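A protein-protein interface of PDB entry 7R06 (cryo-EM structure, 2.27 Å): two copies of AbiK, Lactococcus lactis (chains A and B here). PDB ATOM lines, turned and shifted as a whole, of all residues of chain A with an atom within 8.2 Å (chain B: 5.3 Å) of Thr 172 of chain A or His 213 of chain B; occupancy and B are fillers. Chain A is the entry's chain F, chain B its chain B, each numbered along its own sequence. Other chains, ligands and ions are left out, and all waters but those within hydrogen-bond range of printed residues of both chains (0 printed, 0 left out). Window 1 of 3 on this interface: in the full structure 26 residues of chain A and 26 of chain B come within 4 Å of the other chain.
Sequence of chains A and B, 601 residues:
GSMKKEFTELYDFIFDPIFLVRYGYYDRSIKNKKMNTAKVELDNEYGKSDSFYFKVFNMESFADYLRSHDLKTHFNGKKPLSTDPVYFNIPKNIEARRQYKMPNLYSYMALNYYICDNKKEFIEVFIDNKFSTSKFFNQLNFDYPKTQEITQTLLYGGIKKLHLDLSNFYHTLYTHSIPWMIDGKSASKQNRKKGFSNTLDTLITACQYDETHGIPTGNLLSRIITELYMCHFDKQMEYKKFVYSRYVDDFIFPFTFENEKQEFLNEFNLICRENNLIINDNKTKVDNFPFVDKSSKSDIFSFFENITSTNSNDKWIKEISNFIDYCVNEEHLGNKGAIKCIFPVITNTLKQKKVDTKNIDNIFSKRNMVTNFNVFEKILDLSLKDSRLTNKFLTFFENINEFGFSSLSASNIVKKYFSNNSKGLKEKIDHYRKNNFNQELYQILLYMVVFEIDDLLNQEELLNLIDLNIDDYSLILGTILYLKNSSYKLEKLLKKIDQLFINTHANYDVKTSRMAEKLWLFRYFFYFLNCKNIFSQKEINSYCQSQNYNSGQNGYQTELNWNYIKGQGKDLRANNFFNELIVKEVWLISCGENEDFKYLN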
ATOM      1  N   LEU A 166      24.022  -2.400  28.444  1.00  0.00           N
ATOM      2  CA  LEU A 166      22.807  -3.175  28.624  1.00  0.00           C
ATOM      3  C   LEU A 166      23.066  -4.585  28.114  1.00  0.00           C
ATOM      4  O   LEU A 166      23.643  -4.764  27.038  1.00  0.00           O
ATOM      5  CB  LEU A 166      21.634  -2.534  27.887  1.00  0.00           C
ATOM      6  CG  LEU A 166      21.277  -1.118  28.349  1.00  0.00           C
ATOM      7  CD1 LEU A 166      20.158  -0.534  27.499  1.00  0.00           C
ATOM      8  CD2 LEU A 166      20.925  -1.070  29.826  1.00  0.00           C
ATOM      9  N   SER A 167      22.662  -5.580  28.890  1.00  0.00           N
ATOM     10  CA  SER A 167      22.922  -6.964  28.527  1.00  0.00           C
ATOM     11  C   SER A 167      21.842  -7.478  27.583  1.00  0.00           C
ATOM     12  O   SER A 167      20.649  -7.322  27.853  1.00  0.00           O
ATOM     13  CB  SER A 167      23.000  -7.834  29.779  1.00  0.00           C
ATOM     14  OG  SER A 167      22.039  -7.431  30.731  1.00  0.00           O
ATOM     15  N   ASN A 168      22.272  -8.079  26.472  1.00  0.00           N
ATOM     16  CA  ASN A 168      21.378  -8.733  25.514  1.00  0.00           C
ATOM     17  C   ASN A 168      20.262  -7.792  25.070  1.00  0.00           C
ATOM     18  O   ASN A 168      19.083  -8.151  25.044  1.00  0.00           O
ATOM     19  CB  ASN A 168      20.808 -10.023  26.105  1.00  0.00           C
ATOM     20  CG  ASN A 168      21.877 -10.918  26.694  1.00  0.00           C
ATOM     21  OD1 ASN A 168      21.810 -11.305  27.860  1.00  0.00           O
ATOM     22  ND2 ASN A 168      22.874 -11.253  25.886  1.00  0.00           N
ATOM     23  N   PHE A 169      20.650  -6.562  24.723  1.00  0.00           N
ATOM     24  CA  PHE A 169      19.679  -5.485  24.568  1.00  0.00           C
ATOM     25  C   PHE A 169      18.712  -5.746  23.420  1.00  0.00           C
ATOM     26  O   PHE A 169      17.491  -5.704  23.604  1.00  0.00           O
ATOM     27  CB  PHE A 169      20.409  -4.159  24.366  1.00  0.00           C
ATOM     28  CG  PHE A 169      19.503  -3.019  24.022  1.00  0.00           C
ATOM     29  CD1 PHE A 169      18.402  -2.732  24.804  1.00  0.00           C
ATOM     30  CD2 PHE A 169      19.750  -2.240  22.913  1.00  0.00           C
ATOM     31  CE1 PHE A 169      17.567  -1.686  24.483  1.00  0.00           C
ATOM     32  CE2 PHE A 169      18.921  -1.192  22.595  1.00  0.00           C
ATOM     33  CZ  PHE A 169      17.828  -0.915  23.379  1.00  0.00           C
ATOM     34  N   TYR A 170      19.239  -6.016  22.225  1.00  0.00           N
ATOM     35  CA  TYR A 170      18.381  -6.221  21.060  1.00  0.00           C
ATOM     36  C   TYR A 170      17.545  -7.485  21.199  1.00  0.00           C
ATOM     37  O   TYR A 170      16.382  -7.514  20.790  1.00  0.00           O
ATOM     38  CB  TYR A 170      19.231  -6.298  19.795  1.00  0.00           C
ATOM     39  CG  TYR A 170      19.510  -4.982  19.118  1.00  0.00           C
ATOM     40  CD1 TYR A 170      20.176  -3.963  19.782  1.00  0.00           C
ATOM     41  CD2 TYR A 170      19.169  -4.782  17.788  1.00  0.00           C
ATOM     42  CE1 TYR A 170      20.455  -2.773  19.158  1.00  0.00           C
ATOM     43  CE2 TYR A 170      19.452  -3.591  17.152  1.00  0.00           C
ATOM     44  CZ  TYR A 170      20.096  -2.591  17.845  1.00  0.00           C
ATOM     45  OH  TYR A 170      20.376  -1.401  17.220  1.00  0.00           O
ATOM     46  N   HIS A 171      18.124  -8.532  21.772  1.00  0.00           N
ATOM     47  CA  HIS A 171      17.568  -9.872  21.702  1.00  0.00           C
ATOM     48  C   HIS A 171      16.597 -10.193  22.828  1.00  0.00           C
ATOM     49  O   HIS A 171      15.872 -11.185  22.730  1.00  0.00           O
ATOM     50  CB  HIS A 171      18.717 -10.879  21.686  1.00  0.00           C
ATOM     51  CG  HIS A 171      19.788 -10.528  20.704  1.00  0.00           C
ATOM     52  ND1 HIS A 171      19.623 -10.668  19.342  1.00  0.00           N
ATOM     53  CD2 HIS A 171      21.020  -9.996  20.881  1.00  0.00           C
ATOM     54  CE1 HIS A 171      20.717 -10.261  18.726  1.00  0.00           C
ATOM     55  NE2 HIS A 171      21.580  -9.849  19.637  1.00  0.00           N
ATOM     56  N   THR A 172      16.555  -9.384  23.883  1.00  0.00           N
ATOM     57  CA  THR A 172      15.595  -9.574  24.963  1.00  0.00           C
ATOM     58  C   THR A 172      14.690  -8.368  25.155  1.00  0.00           C
ATOM     59  O   THR A 172      13.908  -8.344  26.108  1.00  0.00           O
ATOM     60  CB  THR A 172      16.311  -9.896  26.279  1.00  0.00           C
ATOM     61  OG1 THR A 172      16.973  -8.725  26.767  1.00  0.00           O
ATOM     62  CG2 THR A 172      17.315 -11.002  26.084  1.00  0.00           C
ATOM     63  N   LEU A 173      14.778  -7.373  24.279  1.00  0.00           N
ATOM     64  CA  LEU A 173      13.953  -6.180  24.399  1.00  0.00           C
ATOM     65  C   LEU A 173      12.479  -6.550  24.330  1.00  0.00           C
ATOM     66  O   LEU A 173      12.019  -7.135  23.346  1.00  0.00           O
ATOM     67  CB  LEU A 173      14.321  -5.185  23.294  1.00  0.00           C
ATOM     68  CG  LEU A 173      13.598  -3.843  23.108  1.00  0.00           C
ATOM     69  CD1 LEU A 173      12.296  -3.969  22.333  1.00  0.00           C
ATOM     70  CD2 LEU A 173      13.359  -3.167  24.446  1.00  0.00           C
ATOM     71  N   TYR A 174      11.739  -6.208  25.376  1.00  0.00           N
ATOM     72  CA  TYR A 174      10.297  -6.403  25.382  1.00  0.00           C
ATOM     73  C   TYR A 174       9.651  -5.383  24.451  1.00  0.00           C
ATOM     74  O   TYR A 174       9.757  -4.177  24.679  1.00  0.00           O
ATOM     75  CB  TYR A 174       9.770  -6.287  26.811  1.00  0.00           C
ATOM     76  CG  TYR A 174       8.291  -6.537  26.972  1.00  0.00           C
ATOM     77  CD1 TYR A 174       7.691  -7.655  26.420  1.00  0.00           C
ATOM     78  CD2 TYR A 174       7.507  -5.687  27.736  1.00  0.00           C
ATOM     79  CE1 TYR A 174       6.346  -7.894  26.579  1.00  0.00           C
ATOM     80  CE2 TYR A 174       6.160  -5.923  27.910  1.00  0.00           C
ATOM     81  CZ  TYR A 174       5.584  -7.027  27.328  1.00  0.00           C
ATOM     82  OH  TYR A 174       4.242  -7.264  27.494  1.00  0.00           O
ATOM     83  N   THR A 175       8.995  -5.869  23.395  1.00  0.00           N
ATOM     84  CA  THR A 175       8.523  -4.975  22.342  1.00  0.00           C
ATOM     85  C   THR A 175       7.365  -4.100  22.802  1.00  0.00           C
ATOM     86  O   THR A 175       7.181  -3.003  22.269  1.00  0.00           O
ATOM     87  CB  THR A 175       8.115  -5.769  21.099  1.00  0.00           C
ATOM     88  OG1 THR A 175       7.212  -6.813  21.470  1.00  0.00           O
ATOM     89  CG2 THR A 175       9.328  -6.366  20.426  1.00  0.00           C
ATOM     90  N   HIS A 176       6.578  -4.552  23.779  1.00  0.00           N
ATOM     91  CA  HIS A 176       5.541  -3.683  24.323  1.00  0.00           C
ATOM     92  C   HIS A 176       6.097  -2.594  25.223  1.00  0.00           C
ATOM     93  O   HIS A 176       5.347  -1.696  25.610  1.00  0.00           O
ATOM     94  CB  HIS A 176       4.487  -4.489  25.080  1.00  0.00           C
ATOM     95  CG  HIS A 176       3.605  -5.308  24.193  1.00  0.00           C
ATOM     96  ND1 HIS A 176       2.788  -4.755  23.233  1.00  0.00           N
ATOM     97  CD2 HIS A 176       3.402  -6.645  24.134  1.00  0.00           C
ATOM     98  CE1 HIS A 176       2.130  -5.717  22.612  1.00  0.00           C
ATOM     99  NE2 HIS A 176       2.481  -6.873  23.143  1.00  0.00           N
ATOM    100  N   SER A 177       7.379  -2.646  25.563  1.00  0.00           N
ATOM    101  CA  SER A 177       8.005  -1.536  26.262  1.00  0.00           C
ATOM    102  C   SER A 177       8.386  -0.396  25.327  1.00  0.00           C
ATOM    103  O   SER A 177       8.758   0.675  25.808  1.00  0.00           O
ATOM    104  CB  SER A 177       9.236  -2.026  27.030  1.00  0.00           C
ATOM    105  OG  SER A 177      10.423  -1.849  26.283  1.00  0.00           O
ATOM    106  N   TRP A 180       5.966   2.300  25.923  1.00  0.00           N
ATOM    107  CA  TRP A 180       6.295   2.890  27.220  1.00  0.00           C
ATOM    108  C   TRP A 180       7.389   3.934  27.079  1.00  0.00           C
ATOM    109  O   TRP A 180       7.286   5.036  27.622  1.00  0.00           O
ATOM    110  CB  TRP A 180       6.755   1.819  28.206  1.00  0.00           C
ATOM    111  CG  TRP A 180       5.827   0.689  28.422  1.00  0.00           C
ATOM    112  CD1 TRP A 180       4.551   0.566  27.967  1.00  0.00           C
ATOM    113  CD2 TRP A 180       6.124  -0.518  29.121  1.00  0.00           C
ATOM    114  NE1 TRP A 180       4.027  -0.637  28.356  1.00  0.00           N
ATOM    115  CE2 TRP A 180       4.977  -1.324  29.066  1.00  0.00           C
ATOM    116  CE3 TRP A 180       7.251  -0.994  29.794  1.00  0.00           C
ATOM    117  CZ2 TRP A 180       4.921  -2.575  29.659  1.00  0.00           C
ATOM    118  CZ3 TRP A 180       7.193  -2.238  30.380  1.00  0.00           C
ATOM    119  CH2 TRP A 180       6.037  -3.013  30.310  1.00  0.00           C
ATOM    120  N   THR A 212       6.950 -11.266  20.959  1.00  0.00           N
ATOM    121  CA  THR A 212       7.200 -10.012  21.648  1.00  0.00           C
ATOM    122  C   THR A 212       8.554  -9.986  22.328  1.00  0.00           C
ATOM    123  O   THR A 212       8.897  -8.988  22.960  1.00  0.00           O
ATOM    124  CB  THR A 212       6.092  -9.744  22.668  1.00  0.00           C
ATOM    125  OG1 THR A 212       5.835 -10.929  23.423  1.00  0.00           O
ATOM    126  CG2 THR A 212       4.822  -9.330  21.966  1.00  0.00           C
ATOM    127  N   HIS A 213       9.330 -11.051  22.203  1.00  0.00           N
ATOM    128  CA  HIS A 213      10.619 -11.175  22.864  1.00  0.00           C
ATOM    129  C   HIS A 213      11.705 -10.770  21.873  1.00  0.00           C
ATOM    130  O   HIS A 213      12.016 -11.520  20.944  1.00  0.00           O
ATOM    131  CB  HIS A 213      10.819 -12.605  23.359  1.00  0.00           C
ATOM    132  CG  HIS A 213      11.921 -12.752  24.359  1.00  0.00           C
ATOM    133  ND1 HIS A 213      11.839 -12.235  25.634  1.00  0.00           N
ATOM    134  CD2 HIS A 213      13.133 -13.346  24.270  1.00  0.00           C
ATOM    135  CE1 HIS A 213      12.950 -12.515  26.290  1.00  0.00           C
ATOM    136  NE2 HIS A 213      13.752 -13.186  25.484  1.00  0.00           N
ATOM    137  N   GLY A 214      12.271  -9.584  22.066  1.00  0.00           N
ATOM    138  CA  GLY A 214      13.353  -9.107  21.235  1.00  0.00           C
ATOM    139  C   GLY A 214      12.892  -8.408  19.968  1.00  0.00           C
ATOM    140  O   GLY A 214      11.715  -8.381  19.611  1.00  0.00           O
ATOM    141  N   ILE A 215      13.871  -7.837  19.274  1.00  0.00           N
ATOM    142  CA  ILE A 215      13.689  -7.051  18.058  1.00  0.00           C
ATOM    143  C   ILE A 215      14.342  -7.818  16.911  1.00  0.00           C
ATOM    144  O   ILE A 215      15.414  -8.404  17.110  1.00  0.00           O
ATOM    145  CB  ILE A 215      14.298  -5.648  18.242  1.00  0.00           C
ATOM    146  CG1 ILE A 215      13.344  -4.738  19.014  1.00  0.00           C
ATOM    147  CG2 ILE A 215      14.695  -5.021  16.928  1.00  0.00           C
ATOM    148  CD1 ILE A 215      12.184  -4.248  18.212  1.00  0.00           C
ATOM    149  N   THR A 217      16.818  -8.515  14.516  1.00  0.00           N
ATOM    150  CA  THR A 217      18.121  -7.883  14.397  1.00  0.00           C
ATOM    151  C   THR A 217      18.787  -8.235  13.071  1.00  0.00           C
ATOM    152  O   THR A 217      18.644  -9.346  12.557  1.00  0.00           O
ATOM    153  CB  THR A 217      19.007  -8.315  15.572  1.00  0.00           C
ATOM    154  OG1 THR A 217      18.380  -7.939  16.803  1.00  0.00           O
ATOM    155  CG2 THR A 217      20.366  -7.659  15.510  1.00  0.00           C
ATOM    156  N   ASN A 275      11.621   0.039  32.405  1.00  0.00           N
ATOM    157  CA  ASN A 275      11.433  -0.448  31.044  1.00  0.00           C
ATOM    158  C   ASN A 275      11.934  -1.877  30.839  1.00  0.00           C
ATOM    159  O   ASN A 275      12.131  -2.296  29.696  1.00  0.00           O
ATOM    160  CB  ASN A 275      12.097   0.511  30.059  1.00  0.00           C
ATOM    161  CG  ASN A 275      11.327   1.808  29.917  1.00  0.00           C
ATOM    162  OD1 ASN A 275      11.588   2.776  30.623  1.00  0.00           O
ATOM    163  ND2 ASN A 275      10.356   1.822  29.017  1.00  0.00           N
ATOM    164  N   ASN A 276      12.122  -2.638  31.919  1.00  0.00           N
ATOM    165  CA  ASN A 276      12.612  -4.021  31.851  1.00  0.00           C
ATOM    166  C   ASN A 276      13.931  -4.118  31.089  1.00  0.00           C
ATOM    167  O   ASN A 276      14.137  -5.021  30.280  1.00  0.00           O
ATOM    168  CB  ASN A 276      11.573  -4.965  31.241  1.00  0.00           C
ATOM    169  CG  ASN A 276      10.293  -5.024  32.044  1.00  0.00           C
ATOM    170  OD1 ASN A 276      10.294  -5.432  33.202  1.00  0.00           O
ATOM    171  ND2 ASN A 276       9.189  -4.642  31.424  1.00  0.00           N
ATOM    172  N   LEU A 277      14.829  -3.180  31.349  1.00  0.00           N
ATOM    173  CA  LEU A 277      16.170  -3.203  30.793  1.00  0.00           C
ATOM    174  C   LEU A 277      17.136  -3.665  31.874  1.00  0.00           C
ATOM    175  O   LEU A 277      16.974  -3.327  33.049  1.00  0.00           O
ATOM    176  CB  LEU A 277      16.563  -1.821  30.271  1.00  0.00           C
ATOM    177  CG  LEU A 277      15.679  -1.260  29.155  1.00  0.00           C
ATOM    178  CD1 LEU A 277      16.083   0.162  28.804  1.00  0.00           C
ATOM    179  CD2 LEU A 277      15.723  -2.150  27.925  1.00  0.00           C
ATOM    180  N   ILE A 278      18.128  -4.456  31.482  1.00  0.00           N
ATOM    181  CA  ILE A 278      19.048  -5.073  32.425  1.00  0.00           C
ATOM    182  C   ILE A 278      20.461  -4.615  32.097  1.00  0.00           C
ATOM    183  O   ILE A 278      20.911  -4.736  30.953  1.00  0.00           O
ATOM    184  CB  ILE A 278      18.940  -6.607  32.398  1.00  0.00           C
ATOM    185  CG1 ILE A 278      17.573  -7.042  32.929  1.00  0.00           C
ATOM    186  CG2 ILE A 278      20.038  -7.235  33.239  1.00  0.00           C
ATOM    187  CD1 ILE A 278      17.333  -8.521  32.858  1.00  0.00           C
ATOM    188  N   LYS B 101       6.064  -9.896  42.046  1.00  0.00           N
ATOM    189  CA  LYS B 101       4.778  -9.440  41.528  1.00  0.00           C
ATOM    190  C   LYS B 101       3.718 -10.292  42.213  1.00  0.00           C
ATOM    191  O   LYS B 101       3.509 -11.447  41.840  1.00  0.00           O
ATOM    192  CB  LYS B 101       4.701  -9.572  40.012  1.00  0.00           C
ATOM    193  CG  LYS B 101       5.592  -8.617  39.249  1.00  0.00           C
ATOM    194  CD  LYS B 101       5.630  -8.972  37.772  1.00  0.00           C
ATOM    195  CE  LYS B 101       6.298  -7.883  36.963  1.00  0.00           C
ATOM    196  NZ  LYS B 101       6.396  -8.221  35.524  1.00  0.00           N
ATOM    197  N   HIS B 171      12.510 -13.630  35.656  1.00  0.00           N
ATOM    198  CA  HIS B 171      12.112 -12.266  35.354  1.00  0.00           C
ATOM    199  C   HIS B 171      12.178 -11.922  33.874  1.00  0.00           C
ATOM    200  O   HIS B 171      11.622 -10.897  33.471  1.00  0.00           O
ATOM    201  CB  HIS B 171      12.985 -11.309  36.162  1.00  0.00           C
ATOM    202  CG  HIS B 171      13.089 -11.689  37.604  1.00  0.00           C
ATOM    203  ND1 HIS B 171      12.050 -11.520  38.495  1.00  0.00           N
ATOM    204  CD2 HIS B 171      14.089 -12.276  38.301  1.00  0.00           C
ATOM    205  CE1 HIS B 171      12.416 -11.964  39.683  1.00  0.00           C
ATOM    206  NE2 HIS B 171      13.649 -12.427  39.593  1.00  0.00           N
ATOM    207  N   THR B 172      12.828 -12.745  33.056  1.00  0.00           N
ATOM    208  CA  THR B 172      12.866 -12.531  31.615  1.00  0.00           C
ATOM    209  C   THR B 172      12.280 -13.700  30.839  1.00  0.00           C
ATOM    210  O   THR B 172      12.354 -13.706  29.607  1.00  0.00           O
ATOM    211  CB  THR B 172      14.297 -12.263  31.140  1.00  0.00           C
ATOM    212  OG1 THR B 172      15.064 -13.469  31.211  1.00  0.00           O
ATOM    213  CG2 THR B 172      14.949 -11.196  31.984  1.00  0.00           C
ATOM    214  N   LEU B 173      11.708 -14.685  31.525  1.00  0.00           N
ATOM    215  CA  LEU B 173      11.134 -15.844  30.856  1.00  0.00           C
ATOM    216  C   LEU B 173      10.022 -15.409  29.913  1.00  0.00           C
ATOM    217  O   LEU B 173       9.043 -14.788  30.333  1.00  0.00           O
ATOM    218  CB  LEU B 173      10.612 -16.833  31.901  1.00  0.00           C
ATOM    219  CG  LEU B 173       9.898 -18.141  31.523  1.00  0.00           C
ATOM    220  CD1 LEU B 173       8.423 -17.946  31.209  1.00  0.00           C
ATOM    221  CD2 LEU B 173      10.603 -18.827  30.366  1.00  0.00           C
ATOM    222  N   THR B 175       6.805 -15.923  28.222  1.00  0.00           N
ATOM    223  CA  THR B 175       5.706 -16.780  28.660  1.00  0.00           C
ATOM    224  C   THR B 175       5.132 -17.611  27.522  1.00  0.00           C
ATOM    225  O   THR B 175       4.588 -18.690  27.768  1.00  0.00           O
ATOM    226  CB  THR B 175       4.597 -15.948  29.308  1.00  0.00           C
ATOM    227  OG1 THR B 175       4.232 -14.873  28.441  1.00  0.00           O
ATOM    228  CG2 THR B 175       5.054 -15.393  30.637  1.00  0.00           C
ATOM    229  N   GLN B 208      -0.380 -10.936  35.270  1.00  0.00           N
ATOM    230  CA  GLN B 208       0.510  -9.778  35.177  1.00  0.00           C
ATOM    231  C   GLN B 208       0.075  -8.801  34.084  1.00  0.00           C
ATOM    232  O   GLN B 208       0.904  -8.170  33.432  1.00  0.00           O
ATOM    233  CB  GLN B 208       1.959 -10.214  34.969  1.00  0.00           C
ATOM    234  CG  GLN B 208       2.165 -11.181  33.824  1.00  0.00           C
ATOM    235  CD  GLN B 208       3.588 -11.671  33.725  1.00  0.00           C
ATOM    236  OE1 GLN B 208       4.523 -10.880  33.646  1.00  0.00           O
ATOM    237  NE2 GLN B 208       3.754 -12.975  33.657  1.00  0.00           N
ATOM    238  N   GLU B 211       1.086  -9.164  30.279  1.00  0.00           N
ATOM    239  CA  GLU B 211       2.491  -8.912  30.033  1.00  0.00           C
ATOM    240  C   GLU B 211       3.143 -10.269  29.809  1.00  0.00           C
ATOM    241  O   GLU B 211       2.955 -11.190  30.608  1.00  0.00           O
ATOM    242  CB  GLU B 211       3.109  -8.176  31.216  1.00  0.00           C
ATOM    243  CG  GLU B 211       2.791  -6.683  31.222  1.00  0.00           C
ATOM    244  CD  GLU B 211       3.974  -5.800  31.514  1.00  0.00           C
ATOM    245  OE1 GLU B 211       3.767  -4.576  31.625  1.00  0.00           O
ATOM    246  OE2 GLU B 211       5.096  -6.315  31.654  1.00  0.00           O
ATOM    247  N   THR B 212       3.882 -10.405  28.716  1.00  0.00           N
ATOM    248  CA  THR B 212       4.479 -11.680  28.359  1.00  0.00           C
ATOM    249  C   THR B 212       5.933 -11.775  28.777  1.00  0.00           C
ATOM    250  O   THR B 212       6.570 -12.797  28.529  1.00  0.00           O
ATOM    251  CB  THR B 212       4.348 -11.916  26.853  1.00  0.00           C
ATOM    252  OG1 THR B 212       4.723 -10.734  26.144  1.00  0.00           O
ATOM    253  CG2 THR B 212       2.923 -12.264  26.499  1.00  0.00           C
ATOM    254  N   HIS B 213       6.462 -10.742  29.414  1.00  0.00           N
ATOM    255  CA  HIS B 213       7.862 -10.684  29.807  1.00  0.00           C
ATOM    256  C   HIS B 213       7.967 -11.120  31.264  1.00  0.00           C
ATOM    257  O   HIS B 213       7.597 -10.368  32.169  1.00  0.00           O
ATOM    258  CB  HIS B 213       8.404  -9.272  29.603  1.00  0.00           C
ATOM    259  CG  HIS B 213       9.897  -9.189  29.619  1.00  0.00           C
ATOM    260  ND1 HIS B 213      10.680  -9.723  28.619  1.00  0.00           N
ATOM    261  CD2 HIS B 213      10.751  -8.646  30.518  1.00  0.00           C
ATOM    262  CE1 HIS B 213      11.952  -9.502  28.896  1.00  0.00           C
ATOM    263  NE2 HIS B 213      12.022  -8.852  30.044  1.00  0.00           N
ATOM    264  N   GLY B 214       8.463 -12.331  31.486  1.00  0.00           N
ATOM    265  CA  GLY B 214       8.671 -12.841  32.822  1.00  0.00           C
ATOM    266  C   GLY B 214       7.443 -13.499  33.428  1.00  0.00           C
ATOM    267  O   GLY B 214       6.337 -13.469  32.890  1.00  0.00           O
ATOM    268  N   ILE B 215       7.667 -14.099  34.591  1.00  0.00           N
ATOM    269  CA  ILE B 215       6.673 -14.858  35.348  1.00  0.00           C
ATOM    270  C   ILE B 215       6.407 -14.101  36.646  1.00  0.00           C
ATOM    271  O   ILE B 215       7.352 -13.565  37.238  1.00  0.00           O
ATOM    272  CB  ILE B 215       7.185 -16.288  35.601  1.00  0.00           C
ATOM    273  CG1 ILE B 215       6.971 -17.169  34.372  1.00  0.00           C
ATOM    274  CG2 ILE B 215       6.557 -16.910  36.825  1.00  0.00           C
ATOM    275  CD1 ILE B 215       5.555 -17.597  34.164  1.00  0.00           C
ATOM    276  N   ILE B 278      18.929 -17.858  28.460  1.00  0.00           N
ATOM    277  CA  ILE B 278      20.271 -17.298  28.402  1.00  0.00           C
ATOM    278  C   ILE B 278      21.064 -17.810  29.594  1.00  0.00           C
ATOM    279  O   ILE B 278      20.622 -17.691  30.743  1.00  0.00           O
ATOM    280  CB  ILE B 278      20.239 -15.760  28.375  1.00  0.00           C
ATOM    281  CG1 ILE B 278      19.615 -15.276  27.066  1.00  0.00           C
ATOM    282  CG2 ILE B 278      21.641 -15.194  28.515  1.00  0.00           C
ATOM    283  CD1 ILE B 278      19.453 -13.786  26.981  1.00  0.00           C
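Of chain B, only His 213 and Ile 278 come within 4 Å of Thr 172 of chain A.
No residue of chain A comes within 4 Å of Gly 214 of chain B.
Of the printed residues of chain A, Thr 212 of chain B touches Tyr 174 and Thr 212.
Of the printed residues of chain B, Trp 180 of chain A touches Glu 211.
Printed residues of chain B within 4 Å of Tyr 174 of chain A: Glu 211 (3.5 Å), Thr 212 (3.3 Å) and His 213 (3.6 Å).
Of the printed residues of chain B, Asn 276 of chain A touches His 213 (3.8 Å).
Of the printed residues of chain B, His 213 of chain A touches Thr 172 (3.6 Å).
The nearest residue of chain A that does not touch His 213 of chain B is His 213 of chain A (4.1 Å).
The side-chain hydroxyl of Thr 212 of chain B lies within hydrogen-bond range of the side-chain hydroxyl of Thr 212 of chain A (2.9 Å).
N of Thr 212 of chain B is in hydrogen-bond range of OH of Tyr 174 of chain A.
Printed residues of chain A that touch a printed residue of chain B: Asn 168, Thr 172, Tyr 174, Trp 180, Thr 212, His 213, Asn 276 and Ile 278.
Hydrophobic or aromatic side chains of chain A within 4 Å of the printed part of chain B: Tyr 174, Trp 180, His 213 and Ile 278.
Printed residues of chain B that touch a printed residue of chain A: Thr 172, Glu 211, Thr 212, His 213 and Ile 278.
Hydrophobic or aromatic side chains of chain B that line the printed part of chain A: His 213 and Ile 278.
Among the printed residues, 11 pairs touch across the chains.
Asn 168 of chain A touches Ile 278 of chain B.
Thr 172 of chain A touches His 213 of chain B (O to CE1, 3.6 Å).
Ile 278 of chain B touches Thr 172 of chain A.
CA of Glu 211 of chain B touches OH of Tyr 174 of chain A, 3.5 Å away.
His 213 of chain B touches Tyr 174 of chain A.
OE1 of Glu 211 of chain B touches CZ2 of Trp 180 of chain A, 3.0 Å away.
His 213 of chain A touches Thr 172 of chain B (CE1 to O, 3.6 Å).
CD2 of His 213 of chain B touches CB of Asn 276 of chain A, 3.8 Å away.
CD1 of Ile 278 of chain A touches CG2 of Thr 172 of chain B (3.7 Å).
The side-chain amide oxygen of Gln 208 of chain B lies close to the backbone carbonyl oxygen of Glu 211 of chain B.
The indole nitrogen of Trp 180 of chain A is in hydrogen-bond range of the backbone carbonyl oxygen of His 176 of chain A.
O of His 213 of chain B lies close to OE1 of Gln 208 of chain B, at 3.4 Å.
The backbone NH (N) of Ser 167 of chain A lies within hydrogen-bond range of the backbone carbonyl oxygen (O) of Ile 278 of chain A, 2.8 Å away.
The backbone carbonyl oxygen (O) of Thr 212 of chain B is in hydrogen-bond range of the side-chain hydroxyl (OG1) of Thr 175 of chain B, 3.1 Å away.
O of Thr 212 of chain A is in hydrogen-bond range of OG1 of Thr 175 of chain A (3.1 Å).
Thr 172 of chain A touches His 213 of chain B, and with the chains exchanged His 213 of chain A touches Thr 172 of chain B.
Thr 172 of chain A touches Ile 278 of chain B, and with the chains exchanged Ile 278 of chain A touches Thr 172 of chain B.
Thr 212 of chain B touches its own counterpart, Thr 212 of chain A.
9 positions are printed for both chains.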
